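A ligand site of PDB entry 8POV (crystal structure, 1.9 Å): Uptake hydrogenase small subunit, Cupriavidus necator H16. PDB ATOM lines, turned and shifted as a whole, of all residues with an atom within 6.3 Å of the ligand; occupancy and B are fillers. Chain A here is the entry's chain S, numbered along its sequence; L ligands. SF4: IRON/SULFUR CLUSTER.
An iron atom (FE1) of the ligand is bound by a ring nitrogen (ND1) of His 187 (2.1 Å).
FE4 of the ligand is bound by SG of Cys 215 (2.3 Å).
SG of Cys 190 is bound to FE3 of the ligand, 2.3 Å away.
N of Leu 216 lies close to S1 of the ligand.
N of Arg 193 lies close to S2 of the ligand.
The side-chain sulfur (SG) of Cys 221 binds an iron atom (FE2) of the ligand (2.3 Å).
The guanidinium group (NH1) of Arg 192 sits at hydrogen-bond distance from the backbone carbonyl oxygen (O) of Phe 214 (2.6 Å).
The backbone carbonyl oxygen (O) of Ile 243 is in hydrogen-bond range of the guanidinium group (NH2) of Arg 192 (3.0 Å).
The backbone NH (N) of Cys 221 lies within hydrogen-bond range of the backbone carbonyl oxygen (O) of Leu 216.
The side-chain sulfur (SG) of Cys 221 sits close to the backbone NH (N) of Gly 223.
The side-chain hydroxyl (OH) of Tyr 191 sits at hydrogen-bond distance from the guanidinium group (NE) of Arg 192 (2.9 Å).
N of Tyr 217 sits close to SG of Cys 215 (3.3 Å).
The backbone carbonyl oxygen (O) of Gly 223 sits at hydrogen-bond distance from the backbone NH (N) of His 187 (3.2 Å).
The backbone carbonyl oxygen (O) of His 187 lies close to the guanidinium group (NH1) of Arg 193 (3.2 Å).
C of Arg 192 touches S2 of the ligand, at 3.8 Å.
Phe 196 touches the ligand (CB to S2, 3.8 Å).
Tyr 217 touches the ligand (CB to S3, 3.9 Å).
Gly 223 touches the ligand.
Ile 243 touches the ligand.
The nearest printed residue that does not touch the ligand is Pro 224 (4.001 Å).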
ATOM      1  N   ILE A 186      17.718 -11.559 -14.402  1.00  0.00           N
ATOM      2  CA  ILE A 186      17.623 -13.010 -14.216  1.00  0.00           C
ATOM      3  C   ILE A 186      16.468 -13.587 -15.042  1.00  0.00           C
ATOM      4  O   ILE A 186      16.600 -14.632 -15.682  1.00  0.00           O
ATOM      5  CB  ILE A 186      17.349 -13.432 -12.753  1.00  0.00           C
ATOM      6  CG1 ILE A 186      18.269 -12.700 -11.757  1.00  0.00           C
ATOM      7  CG2 ILE A 186      17.517 -14.951 -12.604  1.00  0.00           C
ATOM      8  CD1 ILE A 186      19.742 -12.843 -12.034  1.00  0.00           C
ATOM      9  N   HIS A 187      15.339 -12.881 -14.988  1.00  0.00           N
ATOM     10  CA  HIS A 187      14.088 -13.264 -15.660  1.00  0.00           C
ATOM     11  C   HIS A 187      14.216 -13.393 -17.197  1.00  0.00           C
ATOM     12  O   HIS A 187      13.432 -14.115 -17.823  1.00  0.00           O
ATOM     13  CB  HIS A 187      13.012 -12.228 -15.285  1.00  0.00           C
ATOM     14  CG  HIS A 187      11.610 -12.592 -15.704  1.00  0.00           C
ATOM     15  ND1 HIS A 187      10.868 -13.548 -15.062  1.00  0.00           N
ATOM     16  CD2 HIS A 187      10.816 -12.083 -16.679  1.00  0.00           C
ATOM     17  CE1 HIS A 187       9.682 -13.640 -15.623  1.00  0.00           C
ATOM     18  NE2 HIS A 187       9.625 -12.764 -16.611  1.00  0.00           N
ATOM     19  N   ASP A 188      15.190 -12.696 -17.784  1.00  0.00           N
ATOM     20  CA  ASP A 188      15.346 -12.669 -19.256  1.00  0.00           C
ATOM     21  C   ASP A 188      15.608 -14.061 -19.846  1.00  0.00           C
ATOM     22  O   ASP A 188      15.012 -14.436 -20.837  1.00  0.00           O
ATOM     23  CB  ASP A 188      16.475 -11.732 -19.702  1.00  0.00           C
ATOM     24  CG  ASP A 188      16.159 -10.254 -19.454  1.00  0.00           C
ATOM     25  OD1 ASP A 188      14.968  -9.888 -19.360  1.00  0.00           O
ATOM     26  OD2 ASP A 188      17.122  -9.467 -19.366  1.00  0.00           O
ATOM     27  N   CYS A 190      16.011 -16.988 -17.691  1.00  0.00           N
ATOM     28  CA  CYS A 190      15.742 -18.027 -16.694  1.00  0.00           C
ATOM     29  C   CYS A 190      15.076 -19.236 -17.358  1.00  0.00           C
ATOM     30  O   CYS A 190      14.109 -19.080 -18.089  1.00  0.00           O
ATOM     31  CB  CYS A 190      14.878 -17.474 -15.563  1.00  0.00           C
ATOM     32  SG  CYS A 190      14.339 -18.695 -14.336  1.00  0.00           S
ATOM     33  N   TYR A 191      15.601 -20.429 -17.090  1.00  0.00           N
ATOM     34  CA  TYR A 191      15.107 -21.651 -17.723  1.00  0.00           C
ATOM     35  C   TYR A 191      13.649 -21.947 -17.318  1.00  0.00           C
ATOM     36  O   TYR A 191      12.979 -22.755 -17.961  1.00  0.00           O
ATOM     37  CB  TYR A 191      16.025 -22.852 -17.401  1.00  0.00           C
ATOM     38  CG  TYR A 191      15.773 -23.451 -16.037  1.00  0.00           C
ATOM     39  CD1 TYR A 191      16.301 -22.870 -14.892  1.00  0.00           C
ATOM     40  CD2 TYR A 191      14.960 -24.570 -15.885  1.00  0.00           C
ATOM     41  CE1 TYR A 191      16.054 -23.387 -13.638  1.00  0.00           C
ATOM     42  CE2 TYR A 191      14.691 -25.094 -14.624  1.00  0.00           C
ATOM     43  CZ  TYR A 191      15.252 -24.496 -13.514  1.00  0.00           C
ATOM     44  OH  TYR A 191      15.003 -25.001 -12.268  1.00  0.00           O
ATOM     45  N   ARG A 192      13.169 -21.305 -16.257  1.00  0.00           N
ATOM     46  CA  ARG A 192      11.763 -21.481 -15.848  1.00  0.00           C
ATOM     47  C   ARG A 192      10.800 -20.539 -16.579  1.00  0.00           C
ATOM     48  O   ARG A 192       9.599 -20.564 -16.315  1.00  0.00           O
ATOM     49  CB  ARG A 192      11.606 -21.312 -14.334  1.00  0.00           C
ATOM     50  CG  ARG A 192      12.414 -22.316 -13.518  1.00  0.00           C
ATOM     51  CD  ARG A 192      11.901 -22.483 -12.088  1.00  0.00           C
ATOM     52  NE  ARG A 192      12.721 -23.451 -11.365  1.00  0.00           N
ATOM     53  CZ  ARG A 192      12.341 -24.119 -10.276  1.00  0.00           C
ATOM     54  NH1 ARG A 192      11.148 -23.943  -9.737  1.00  0.00           N
ATOM     55  NH2 ARG A 192      13.188 -24.987  -9.719  1.00  0.00           N
ATOM     56  N   ARG A 193      11.308 -19.725 -17.494  1.00  0.00           N
ATOM     57  CA  ARG A 193      10.463 -18.750 -18.176  1.00  0.00           C
ATOM     58  C   ARG A 193       9.219 -19.363 -18.839  1.00  0.00           C
ATOM     59  O   ARG A 193       8.120 -18.847 -18.665  1.00  0.00           O
ATOM     60  CB  ARG A 193      11.250 -17.921 -19.202  1.00  0.00           C
ATOM     61  CG  ARG A 193      11.783 -16.609 -18.649  1.00  0.00           C
ATOM     62  CD  ARG A 193      10.664 -15.679 -18.178  1.00  0.00           C
ATOM     63  NE  ARG A 193       9.761 -15.253 -19.244  1.00  0.00           N
ATOM     64  CZ  ARG A 193       9.962 -14.201 -20.030  1.00  0.00           C
ATOM     65  NH1 ARG A 193      11.052 -13.442 -19.911  1.00  0.00           N
ATOM     66  NH2 ARG A 193       9.065 -13.889 -20.957  1.00  0.00           N
ATOM     67  N   PRO A 194       9.404 -20.447 -19.605  1.00  0.00           N
ATOM     68  CA  PRO A 194       8.232 -21.072 -20.224  1.00  0.00           C
ATOM     69  C   PRO A 194       7.070 -21.263 -19.247  1.00  0.00           C
ATOM     70  O   PRO A 194       5.915 -21.036 -19.621  1.00  0.00           O
ATOM     71  CB  PRO A 194       8.784 -22.414 -20.715  1.00  0.00           C
ATOM     72  CG  PRO A 194      10.195 -22.078 -21.087  1.00  0.00           C
ATOM     73  CD  PRO A 194      10.647 -21.087 -20.049  1.00  0.00           C
ATOM     74  N   PHE A 196       6.524 -19.482 -16.366  1.00  0.00           N
ATOM     75  CA  PHE A 196       6.019 -18.134 -16.130  1.00  0.00           C
ATOM     76  C   PHE A 196       5.102 -17.655 -17.269  1.00  0.00           C
ATOM     77  O   PHE A 196       4.033 -17.106 -17.024  1.00  0.00           O
ATOM     78  CB  PHE A 196       7.177 -17.139 -15.963  1.00  0.00           C
ATOM     79  CG  PHE A 196       6.736 -15.716 -15.771  1.00  0.00           C
ATOM     80  CD1 PHE A 196       6.491 -14.903 -16.865  1.00  0.00           C
ATOM     81  CD2 PHE A 196       6.583 -15.192 -14.497  1.00  0.00           C
ATOM     82  CE1 PHE A 196       6.080 -13.593 -16.697  1.00  0.00           C
ATOM     83  CE2 PHE A 196       6.171 -13.881 -14.315  1.00  0.00           C
ATOM     84  CZ  PHE A 196       5.928 -13.080 -15.416  1.00  0.00           C
ATOM     85  N   PHE A 201       2.906 -21.895 -11.804  1.00  0.00           N
ATOM     86  CA  PHE A 201       3.615 -21.388 -10.647  1.00  0.00           C
ATOM     87  C   PHE A 201       3.593 -22.331  -9.466  1.00  0.00           C
ATOM     88  O   PHE A 201       2.600 -23.008  -9.240  1.00  0.00           O
ATOM     89  CB  PHE A 201       2.976 -20.090 -10.191  1.00  0.00           C
ATOM     90  CG  PHE A 201       2.975 -19.009 -11.228  1.00  0.00           C
ATOM     91  CD1 PHE A 201       4.154 -18.352 -11.543  1.00  0.00           C
ATOM     92  CD2 PHE A 201       1.798 -18.634 -11.856  1.00  0.00           C
ATOM     93  CE1 PHE A 201       4.165 -17.352 -12.499  1.00  0.00           C
ATOM     94  CE2 PHE A 201       1.800 -17.615 -12.805  1.00  0.00           C
ATOM     95  CZ  PHE A 201       2.987 -16.978 -13.127  1.00  0.00           C
ATOM     96  N   PHE A 214       8.252 -25.569 -11.740  1.00  0.00           N
ATOM     97  CA  PHE A 214       7.430 -24.419 -12.137  1.00  0.00           C
ATOM     98  C   PHE A 214       8.017 -23.111 -11.605  1.00  0.00           C
ATOM     99  O   PHE A 214       8.836 -23.109 -10.683  1.00  0.00           O
ATOM    100  CB  PHE A 214       5.977 -24.596 -11.665  1.00  0.00           C
ATOM    101  CG  PHE A 214       5.142 -25.504 -12.533  1.00  0.00           C
ATOM    102  CD1 PHE A 214       5.725 -26.390 -13.443  1.00  0.00           C
ATOM    103  CD2 PHE A 214       3.762 -25.501 -12.421  1.00  0.00           C
ATOM    104  CE1 PHE A 214       4.953 -27.219 -14.228  1.00  0.00           C
ATOM    105  CE2 PHE A 214       2.980 -26.340 -13.206  1.00  0.00           C
ATOM    106  CZ  PHE A 214       3.576 -27.199 -14.102  1.00  0.00           C
ATOM    107  N   CYS A 215       7.591 -22.019 -12.229  1.00  0.00           N
ATOM    108  CA  CYS A 215       8.111 -20.689 -11.925  1.00  0.00           C
ATOM    109  C   CYS A 215       7.921 -20.345 -10.447  1.00  0.00           C
ATOM    110  O   CYS A 215       6.957 -20.778  -9.805  1.00  0.00           O
ATOM    111  CB  CYS A 215       7.427 -19.652 -12.812  1.00  0.00           C
ATOM    112  SG  CYS A 215       7.744 -17.927 -12.369  1.00  0.00           S
ATOM    113  N   LEU A 216       8.854 -19.566  -9.913  1.00  0.00           N
ATOM    114  CA  LEU A 216       8.881 -19.264  -8.487  1.00  0.00           C
ATOM    115  C   LEU A 216       8.389 -17.857  -8.161  1.00  0.00           C
ATOM    116  O   LEU A 216       8.595 -17.381  -7.051  1.00  0.00           O
ATOM    117  CB  LEU A 216      10.303 -19.446  -7.948  1.00  0.00           C
ATOM    118  CG  LEU A 216      10.839 -20.881  -7.983  1.00  0.00           C
ATOM    119  CD1 LEU A 216      12.341 -20.890  -7.789  1.00  0.00           C
ATOM    120  CD2 LEU A 216      10.145 -21.745  -6.940  1.00  0.00           C
ATOM    121  N   TYR A 217       7.737 -17.210  -9.126  1.00  0.00           N
ATOM    122  CA  TYR A 217       7.234 -15.835  -8.969  1.00  0.00           C
ATOM    123  C   TYR A 217       6.354 -15.670  -7.725  1.00  0.00           C
ATOM    124  O   TYR A 217       6.551 -14.757  -6.935  1.00  0.00           O
ATOM    125  CB  TYR A 217       6.453 -15.397 -10.217  1.00  0.00           C
ATOM    126  CG  TYR A 217       6.013 -13.941 -10.225  1.00  0.00           C
ATOM    127  CD1 TYR A 217       6.823 -12.941 -10.762  1.00  0.00           C
ATOM    128  CD2 TYR A 217       4.766 -13.568  -9.721  1.00  0.00           C
ATOM    129  CE1 TYR A 217       6.417 -11.620 -10.779  1.00  0.00           C
ATOM    130  CE2 TYR A 217       4.348 -12.245  -9.745  1.00  0.00           C
ATOM    131  CZ  TYR A 217       5.168 -11.276 -10.281  1.00  0.00           C
ATOM    132  OH  TYR A 217       4.740  -9.962 -10.291  1.00  0.00           O
ATOM    133  N   CYS A 221      10.056 -14.698  -6.028  1.00  0.00           N
ATOM    134  CA  CYS A 221      11.232 -14.529  -6.885  1.00  0.00           C
ATOM    135  C   CYS A 221      11.351 -13.112  -7.409  1.00  0.00           C
ATOM    136  O   CYS A 221      10.422 -12.577  -8.005  1.00  0.00           O
ATOM    137  CB  CYS A 221      11.191 -15.531  -8.052  1.00  0.00           C
ATOM    138  SG  CYS A 221      12.647 -15.463  -9.121  1.00  0.00           S
ATOM    139  N   LYS A 222      12.502 -12.484  -7.165  1.00  0.00           N
ATOM    140  CA  LYS A 222      12.744 -11.110  -7.601  1.00  0.00           C
ATOM    141  C   LYS A 222      13.568 -11.067  -8.888  1.00  0.00           C
ATOM    142  O   LYS A 222      14.137 -10.027  -9.238  1.00  0.00           O
ATOM    143  CB  LYS A 222      13.444 -10.321  -6.490  1.00  0.00           C
ATOM    144  CG  LYS A 222      12.632 -10.214  -5.207  1.00  0.00           C
ATOM    145  CD  LYS A 222      11.200  -9.762  -5.466  1.00  0.00           C
ATOM    146  CE  LYS A 222      10.467  -9.452  -4.176  1.00  0.00           C
ATOM    147  NZ  LYS A 222      10.327 -10.635  -3.278  1.00  0.00           N
ATOM    148  N   GLY A 223      13.630 -12.184  -9.597  1.00  0.00           N
ATOM    149  CA  GLY A 223      14.349 -12.256 -10.882  1.00  0.00           C
ATOM    150  C   GLY A 223      13.894 -11.225 -11.901  1.00  0.00           C
ATOM    151  O   GLY A 223      14.725 -10.718 -12.660  1.00  0.00           O
ATOM    152  N   PRO A 224      12.586 -10.894 -11.927  1.00  0.00           N
ATOM    153  CA  PRO A 224      12.107  -9.897 -12.888  1.00  0.00           C
ATOM    154  C   PRO A 224      12.637  -8.480 -12.714  1.00  0.00           C
ATOM    155  O   PRO A 224      12.518  -7.690 -13.636  1.00  0.00           O
ATOM    156  CB  PRO A 224      10.584  -9.917 -12.684  1.00  0.00           C
ATOM    157  CG  PRO A 224      10.304 -11.281 -12.157  1.00  0.00           C
ATOM    158  CD  PRO A 224      11.463 -11.578 -11.256  1.00  0.00           C
ATOM    159  N   PHE A 241      22.013 -22.342  -9.875  1.00  0.00           N
ATOM    160  CA  PHE A 241      21.744 -21.017  -9.360  1.00  0.00           C
ATOM    161  C   PHE A 241      20.484 -21.059  -8.523  1.00  0.00           C
ATOM    162  O   PHE A 241      19.760 -22.070  -8.543  1.00  0.00           O
ATOM    163  CB  PHE A 241      21.749 -19.933 -10.460  1.00  0.00           C
ATOM    164  CG  PHE A 241      20.516 -19.873 -11.318  1.00  0.00           C
ATOM    165  CD1 PHE A 241      20.167 -20.935 -12.146  1.00  0.00           C
ATOM    166  CD2 PHE A 241      19.756 -18.716 -11.361  1.00  0.00           C
ATOM    167  CE1 PHE A 241      19.067 -20.858 -12.968  1.00  0.00           C
ATOM    168  CE2 PHE A 241      18.648 -18.632 -12.183  1.00  0.00           C
ATOM    169  CZ  PHE A 241      18.306 -19.700 -12.983  1.00  0.00           C
ATOM    170  N   ILE A 243      17.411 -20.218  -8.424  1.00  0.00           N
ATOM    171  CA  ILE A 243      16.169 -20.700  -9.014  1.00  0.00           C
ATOM    172  C   ILE A 243      16.222 -22.175  -9.420  1.00  0.00           C
ATOM    173  O   ILE A 243      15.254 -22.899  -9.235  1.00  0.00           O
ATOM    174  CB  ILE A 243      15.761 -19.812 -10.190  1.00  0.00           C
ATOM    175  CG1 ILE A 243      15.316 -18.447  -9.650  1.00  0.00           C
ATOM    176  CG2 ILE A 243      14.634 -20.458 -11.000  1.00  0.00           C
ATOM    177  CD1 ILE A 243      15.601 -17.292 -10.573  1.00  0.00           C
ATOM    178  N   GLY A 248      13.476 -18.831  -4.971  1.00  0.00           N
ATOM    179  CA  GLY A 248      13.392 -17.639  -5.787  1.00  0.00           C
ATOM    180  C   GLY A 248      14.582 -16.736  -5.559  1.00  0.00           C
ATOM    181  O   GLY A 248      15.247 -16.766  -4.517  1.00  0.00           O
ATOM    182  N   CYS A 249      14.873 -15.914  -6.555  1.00  0.00           N
ATOM    183  CA  CYS A 249      15.879 -14.886  -6.418  1.00  0.00           C
ATOM    184  C   CYS A 249      15.392 -13.941  -5.319  1.00  0.00           C
ATOM    185  O   CYS A 249      14.204 -13.600  -5.266  1.00  0.00           O
ATOM    186  CB  CYS A 249      16.065 -14.167  -7.751  1.00  0.00           C
ATOM    187  SG  CYS A 249      17.154 -12.729  -7.707  1.00  0.00           S
HETATM  188 FE1  SF4 L   1      11.237 -15.152 -13.740  1.00  0.00          FE
HETATM  189 FE2  SF4 L   1      11.925 -16.121 -11.150  1.00  0.00          FE
HETATM  190 FE3  SF4 L   1      12.617 -17.478 -13.387  1.00  0.00          FE
HETATM  191 FE4  SF4 L   1       9.931 -17.365 -12.691  1.00  0.00          FE
HETATM  192  S1  SF4 L   1      11.606 -18.359 -11.498  1.00  0.00           S
HETATM  193  S2  SF4 L   1      10.815 -17.159 -14.762  1.00  0.00           S
HETATM  194  S3  SF4 L   1       9.951 -15.252 -11.819  1.00  0.00           S
HETATM  195  S4  SF4 L   1      13.353 -15.409 -12.809  1.00  0.00           S
